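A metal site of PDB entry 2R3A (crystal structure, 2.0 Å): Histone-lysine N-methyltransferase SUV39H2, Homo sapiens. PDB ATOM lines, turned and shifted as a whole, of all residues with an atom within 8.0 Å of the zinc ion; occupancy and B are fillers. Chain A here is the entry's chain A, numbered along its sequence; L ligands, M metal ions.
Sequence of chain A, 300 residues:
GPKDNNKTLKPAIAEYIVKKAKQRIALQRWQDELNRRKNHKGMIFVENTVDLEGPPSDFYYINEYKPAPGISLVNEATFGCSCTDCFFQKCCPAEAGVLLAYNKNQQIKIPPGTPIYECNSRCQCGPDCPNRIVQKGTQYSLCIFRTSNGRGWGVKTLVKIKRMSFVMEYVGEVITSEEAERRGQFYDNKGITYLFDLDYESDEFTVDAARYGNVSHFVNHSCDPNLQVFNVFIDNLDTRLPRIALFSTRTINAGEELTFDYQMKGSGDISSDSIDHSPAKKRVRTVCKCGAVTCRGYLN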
ATOM      1  N   ARG A 151      21.822  26.905  25.350  1.00  0.00           N
ATOM      2  CA  ARG A 151      22.474  25.778  26.008  1.00  0.00           C
ATOM      3  C   ARG A 151      23.396  26.230  27.174  1.00  0.00           C
ATOM      4  O   ARG A 151      24.226  25.441  27.633  1.00  0.00           O
ATOM      5  CB  ARG A 151      23.253  24.938  24.997  1.00  0.00           C
ATOM      6  CG  ARG A 151      22.350  24.136  24.033  1.00  0.00           C
ATOM      7  CD  ARG A 151      23.161  23.499  22.888  1.00  0.00           C
ATOM      8  NE  ARG A 151      23.784  24.546  22.082  1.00  0.00           N
ATOM      9  CZ  ARG A 151      25.098  24.682  21.895  1.00  0.00           C
ATOM     10  NH1 ARG A 151      25.968  23.821  22.415  1.00  0.00           N
ATOM     11  NH2 ARG A 151      25.550  25.705  21.168  1.00  0.00           N
ATOM     12  N   HIS A 221      26.432  18.501  25.834  1.00  0.00           N
ATOM     13  CA  HIS A 221      26.086  17.269  25.143  1.00  0.00           C
ATOM     14  C   HIS A 221      25.916  17.495  23.674  1.00  0.00           C
ATOM     15  O   HIS A 221      25.297  18.475  23.238  1.00  0.00           O
ATOM     16  CB  HIS A 221      24.748  16.745  25.676  1.00  0.00           C
ATOM     17  CG  HIS A 221      24.158  15.677  24.819  1.00  0.00           C
ATOM     18  ND1 HIS A 221      24.496  14.343  24.947  1.00  0.00           N
ATOM     19  CD2 HIS A 221      23.300  15.747  23.780  1.00  0.00           C
ATOM     20  CE1 HIS A 221      23.847  13.650  24.027  1.00  0.00           C
ATOM     21  NE2 HIS A 221      23.139  14.478  23.295  1.00  0.00           N
ATOM     22  N   SER A 222      26.415  16.556  22.889  1.00  0.00           N
ATOM     23  CA  SER A 222      26.026  16.493  21.491  1.00  0.00           C
ATOM     24  C   SER A 222      25.714  15.082  21.060  1.00  0.00           C
ATOM     25  O   SER A 222      26.320  14.136  21.562  1.00  0.00           O
ATOM     26  CB  SER A 222      27.130  17.025  20.569  1.00  0.00           C
ATOM     27  OG  SER A 222      26.804  16.811  19.218  1.00  0.00           O
ATOM     28  N   CYS A 223      24.815  14.961  20.080  1.00  0.00           N
ATOM     29  CA  CYS A 223      24.430  13.661  19.451  1.00  0.00           C
ATOM     30  C   CYS A 223      25.421  13.192  18.374  1.00  0.00           C
ATOM     31  O   CYS A 223      25.404  12.005  17.939  1.00  0.00           O
ATOM     32  CB  CYS A 223      23.011  13.760  18.899  1.00  0.00           C
ATOM     33  SG  CYS A 223      21.740  14.154  20.184  1.00  0.00           S
ATOM     34  N   ASP A 224      26.285  14.114  17.964  1.00  0.00           N
ATOM     35  CA  ASP A 224      27.440  13.816  17.135  1.00  0.00           C
ATOM     36  C   ASP A 224      28.679  14.503  17.774  1.00  0.00           C
ATOM     37  O   ASP A 224      29.163  15.538  17.295  1.00  0.00           O
ATOM     38  CB  ASP A 224      27.225  14.298  15.652  1.00  0.00           C
ATOM     39  CG  ASP A 224      28.324  13.759  14.696  1.00  0.00           C
ATOM     40  OD1 ASP A 224      29.099  12.887  15.124  1.00  0.00           O
ATOM     41  OD2 ASP A 224      28.414  14.166  13.529  1.00  0.00           O
ATOM     42  N   VAL A 287      15.110  18.875  26.136  1.00  0.00           N
ATOM     43  CA  VAL A 287      15.206  18.871  24.694  1.00  0.00           C
ATOM     44  C   VAL A 287      16.653  19.178  24.281  1.00  0.00           C
ATOM     45  O   VAL A 287      17.277  20.117  24.778  1.00  0.00           O
ATOM     46  CB  VAL A 287      14.171  19.841  24.039  1.00  0.00           C
ATOM     47  CG1 VAL A 287      14.409  19.979  22.547  1.00  0.00           C
ATOM     48  CG2 VAL A 287      12.693  19.384  24.327  1.00  0.00           C
ATOM     49  N   CYS A 288      17.179  18.348  23.395  1.00  0.00           N
ATOM     50  CA  CYS A 288      18.518  18.542  22.889  1.00  0.00           C
ATOM     51  C   CYS A 288      18.576  19.596  21.800  1.00  0.00           C
ATOM     52  O   CYS A 288      17.823  19.534  20.803  1.00  0.00           O
ATOM     53  CB  CYS A 288      19.055  17.233  22.336  1.00  0.00           C
ATOM     54  SG  CYS A 288      20.774  17.482  21.928  1.00  0.00           S
ATOM     55  N   LYS A 289      19.456  20.584  21.999  1.00  0.00           N
ATOM     56  CA  LYS A 289      19.644  21.645  21.004  1.00  0.00           C
ATOM     57  C   LYS A 289      21.043  21.570  20.368  1.00  0.00           C
ATOM     58  O   LYS A 289      21.635  22.585  19.940  1.00  0.00           O
ATOM     59  CB  LYS A 289      19.343  23.036  21.627  1.00  0.00           C
ATOM     60  CG  LYS A 289      17.879  23.176  22.154  1.00  0.00           C
ATOM     61  CD  LYS A 289      17.518  24.604  22.547  1.00  0.00           C
ATOM     62  CE  LYS A 289      17.320  25.462  21.245  1.00  0.00           C
ATOM     63  NZ  LYS A 289      16.595  26.775  21.452  1.00  0.00           N
ATOM     64  N   CYS A 290      21.566  20.352  20.270  1.00  0.00           N
ATOM     65  CA  CYS A 290      22.947  20.191  19.796  1.00  0.00           C
ATOM     66  C   CYS A 290      23.133  20.660  18.354  1.00  0.00           C
ATOM     67  O   CYS A 290      24.240  21.054  17.961  1.00  0.00           O
ATOM     68  CB  CYS A 290      23.483  18.756  20.018  1.00  0.00           C
ATOM     69  SG  CYS A 290      22.914  17.472  18.782  1.00  0.00           S
ATOM     70  N   GLY A 291      22.047  20.630  17.570  1.00  0.00           N
ATOM     71  CA  GLY A 291      22.058  21.123  16.189  1.00  0.00           C
ATOM     72  C   GLY A 291      22.454  20.139  15.102  1.00  0.00           C
ATOM     73  O   GLY A 291      22.452  20.483  13.920  1.00  0.00           O
ATOM     74  N   ALA A 292      22.893  18.950  15.504  1.00  0.00           N
ATOM     75  CA  ALA A 292      23.251  17.884  14.604  1.00  0.00           C
ATOM     76  C   ALA A 292      22.071  17.493  13.750  1.00  0.00           C
ATOM     77  O   ALA A 292      20.968  17.298  14.251  1.00  0.00           O
ATOM     78  CB  ALA A 292      23.708  16.633  15.407  1.00  0.00           C
ATOM     79  N   VAL A 293      22.310  17.289  12.472  1.00  0.00           N
ATOM     80  CA  VAL A 293      21.307  16.662  11.608  1.00  0.00           C
ATOM     81  C   VAL A 293      20.714  15.373  12.238  1.00  0.00           C
ATOM     82  O   VAL A 293      19.507  15.141  12.225  1.00  0.00           O
ATOM     83  CB  VAL A 293      21.898  16.439  10.218  1.00  0.00           C
ATOM     84  CG1 VAL A 293      21.117  15.413   9.436  1.00  0.00           C
ATOM     85  CG2 VAL A 293      21.952  17.797   9.490  1.00  0.00           C
ATOM     86  N   THR A 294      21.564  14.564  12.834  1.00  0.00           N
ATOM     87  CA  THR A 294      21.109  13.317  13.433  1.00  0.00           C
ATOM     88  C   THR A 294      20.695  13.451  14.921  1.00  0.00           C
ATOM     89  O   THR A 294      20.674  12.455  15.648  1.00  0.00           O
ATOM     90  CB  THR A 294      22.261  12.309  13.351  1.00  0.00           C
ATOM     91  OG1 THR A 294      23.436  12.926  13.921  1.00  0.00           O
ATOM     92  CG2 THR A 294      22.550  11.928  11.881  1.00  0.00           C
ATOM     93  N   CYS A 295      20.404  14.673  15.364  1.00  0.00           N
ATOM     94  CA  CYS A 295      20.034  14.928  16.745  1.00  0.00           C
ATOM     95  C   CYS A 295      18.948  13.943  17.240  1.00  0.00           C
ATOM     96  O   CYS A 295      17.965  13.685  16.540  1.00  0.00           O
ATOM     97  CB  CYS A 295      19.569  16.379  16.931  1.00  0.00           C
ATOM     98  SG  CYS A 295      19.098  16.737  18.629  1.00  0.00           S
ATOM     99  N   ARG A 296      19.132  13.395  18.444  1.00  0.00           N
ATOM    100  CA  ARG A 296      18.156  12.425  18.975  1.00  0.00           C
ATOM    101  C   ARG A 296      16.945  13.085  19.640  1.00  0.00           C
ATOM    102  O   ARG A 296      15.940  12.409  19.981  1.00  0.00           O
ATOM    103  CB  ARG A 296      18.832  11.426  19.911  1.00  0.00           C
ATOM    104  CG  ARG A 296      20.044  10.726  19.281  1.00  0.00           C
ATOM    105  CD  ARG A 296      20.572   9.587  20.150  1.00  0.00           C
ATOM    106  NE  ARG A 296      20.986   9.992  21.510  1.00  0.00           N
ATOM    107  CZ  ARG A 296      22.251  10.197  21.898  1.00  0.00           C
ATOM    108  NH1 ARG A 296      23.255  10.049  21.048  1.00  0.00           N
ATOM    109  NH2 ARG A 296      22.487  10.523  23.168  1.00  0.00           N
ATOM    110  N   GLY A 297      17.050  14.391  19.859  1.00  0.00           N
ATOM    111  CA  GLY A 297      15.919  15.222  20.304  1.00  0.00           C
ATOM    112  C   GLY A 297      15.918  15.512  21.782  1.00  0.00           C
ATOM    113  O   GLY A 297      15.346  16.519  22.236  1.00  0.00           O
ATOM    114  N   TYR A 298      16.536  14.627  22.548  1.00  0.00           N
ATOM    115  CA  TYR A 298      16.529  14.707  23.999  1.00  0.00           C
ATOM    116  C   TYR A 298      17.880  14.341  24.590  1.00  0.00           C
ATOM    117  O   TYR A 298      18.588  13.516  24.019  1.00  0.00           O
ATOM    118  CB  TYR A 298      15.470  13.747  24.546  1.00  0.00           C
ATOM    119  CG  TYR A 298      14.042  14.181  24.248  1.00  0.00           C
ATOM    120  CD1 TYR A 298      13.418  15.178  25.003  1.00  0.00           C
ATOM    121  CD2 TYR A 298      13.305  13.590  23.207  1.00  0.00           C
ATOM    122  CE1 TYR A 298      12.095  15.578  24.766  1.00  0.00           C
ATOM    123  CE2 TYR A 298      11.963  13.991  22.933  1.00  0.00           C
ATOM    124  CZ  TYR A 298      11.368  14.997  23.723  1.00  0.00           C
ATOM    125  OH  TYR A 298      10.046  15.417  23.491  1.00  0.00           O
ATOM    126  N   LEU A 299      18.219  14.924  25.738  1.00  0.00           N
ATOM    127  CA  LEU A 299      19.453  14.566  26.470  1.00  0.00           C
ATOM    128  C   LEU A 299      19.289  13.302  27.327  1.00  0.00           C
ATOM    129  O   LEU A 299      20.269  12.568  27.525  1.00  0.00           O
ATOM    130  CB  LEU A 299      19.954  15.720  27.369  1.00  0.00           C
ATOM    131  CG  LEU A 299      20.160  17.145  26.850  1.00  0.00           C
ATOM    132  CD1 LEU A 299      21.005  17.935  27.832  1.00  0.00           C
ATOM    133  CD2 LEU A 299      20.822  17.150  25.526  1.00  0.00           C
HETATM  134  N1  LIG L   1      25.448  24.347  29.682  1.00  0.00           N
HETATM  135  C1  LIG L   1      25.947  24.058  31.050  1.00  0.00           C
HETATM  136  C2  LIG L   1      26.044  25.336  31.922  1.00  0.00           C
HETATM  137  O1  LIG L   1      25.571  26.401  31.560  1.00  0.00           O
HETATM  138  O2  LIG L   1      26.602  25.347  32.991  1.00  0.00           O
HETATM  139  C3  LIG L   1      27.234  23.251  31.002  1.00  0.00           C
HETATM  140  C4  LIG L   1      27.024  21.738  30.910  1.00  0.00           C
HETATM  141  S1  LIG L   1      25.989  21.025  32.238  1.00  0.00           S
HETATM  142  C5  LIG L   1      27.127  19.637  32.546  1.00  0.00           C
HETATM  143  C6  LIG L   1      24.627  20.212  31.331  1.00  0.00           C
HETATM  144  C7  LIG L   1      23.416  21.129  31.119  1.00  0.00           C
HETATM  145  O3  LIG L   1      23.670  22.032  30.049  1.00  0.00           O
HETATM  146  C8  LIG L   1      22.128  20.426  30.766  1.00  0.00           C
HETATM  147  O4  LIG L   1      21.320  20.107  31.871  1.00  0.00           O
HETATM  148  C9  LIG L   1      21.430  21.458  29.902  1.00  0.00           C
HETATM  149  O5  LIG L   1      20.885  22.479  30.703  1.00  0.00           O
HETATM  150  C10 LIG L   1      22.567  22.141  29.176  1.00  0.00           C
HETATM  151  N2  LIG L   1      22.876  21.430  27.914  1.00  0.00           N
HETATM  152  C11 LIG L   1      24.039  20.768  27.599  1.00  0.00           C
HETATM  153  N3  LIG L   1      23.932  20.268  26.368  1.00  0.00           N
HETATM  154  C12 LIG L   1      22.746  20.610  25.866  1.00  0.00           C
HETATM  155  C13 LIG L   1      22.102  20.358  24.638  1.00  0.00           C
HETATM  156  N4  LIG L   1      22.700  19.665  23.658  1.00  0.00           N
HETATM  157  N5  LIG L   1      20.828  20.862  24.466  1.00  0.00           N
HETATM  158  C14 LIG L   1      20.177  21.581  25.437  1.00  0.00           C
HETATM  159  N6  LIG L   1      20.814  21.842  26.634  1.00  0.00           N
HETATM  160  C15 LIG L   1      22.059  21.342  26.837  1.00  0.00           C
HETATM  161 ZN    ZN M   1      21.131  16.455  19.858  1.00  0.00          ZN
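The side-chain sulfur of Cys 288 lies close to a nitrogen (N4) of the ligand (3.4 Å).
A nitrogen (N3) of the ligand is in hydrogen-bond range of the backbone NH (N) of His 221.
N4 of the ligand is in hydrogen-bond range of O of His 221 (2.9 Å).
N of Lys 289 sits at hydrogen-bond distance from N5 of the ligand (2.8 Å).
O of Arg 151 sits at hydrogen-bond distance from N1 of the ligand (2.6 Å).
The side-chain sulfur of Cys 290 sits close to the backbone NH of Ala 292, 3.6 Å away.
The backbone NH (N) of Cys 288 is in hydrogen-bond range of the backbone carbonyl oxygen (O) of Gly 297 (2.8 Å).
SG of Cys 295 sits close to N of Gly 297, 3.3 Å away.
SG of Cys 223 sits close to N of Arg 296, at 3.2 Å.
SG of Cys 223 lies close to NE2 of His 221 (3.4 Å).
Arg 296 touches the zinc ion.
The nearest printed residue that does not touch the zinc ion is His 221 (4.4 Å).
The zinc ion is bound by SG of Cys 290 (2.3 Å), SG of Cys 288 (2.3 Å), SG of Cys 295 (2.4 Å) and SG of Cys 223 (2.4 Å).
The zinc ion has four donor atoms within binding distance.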
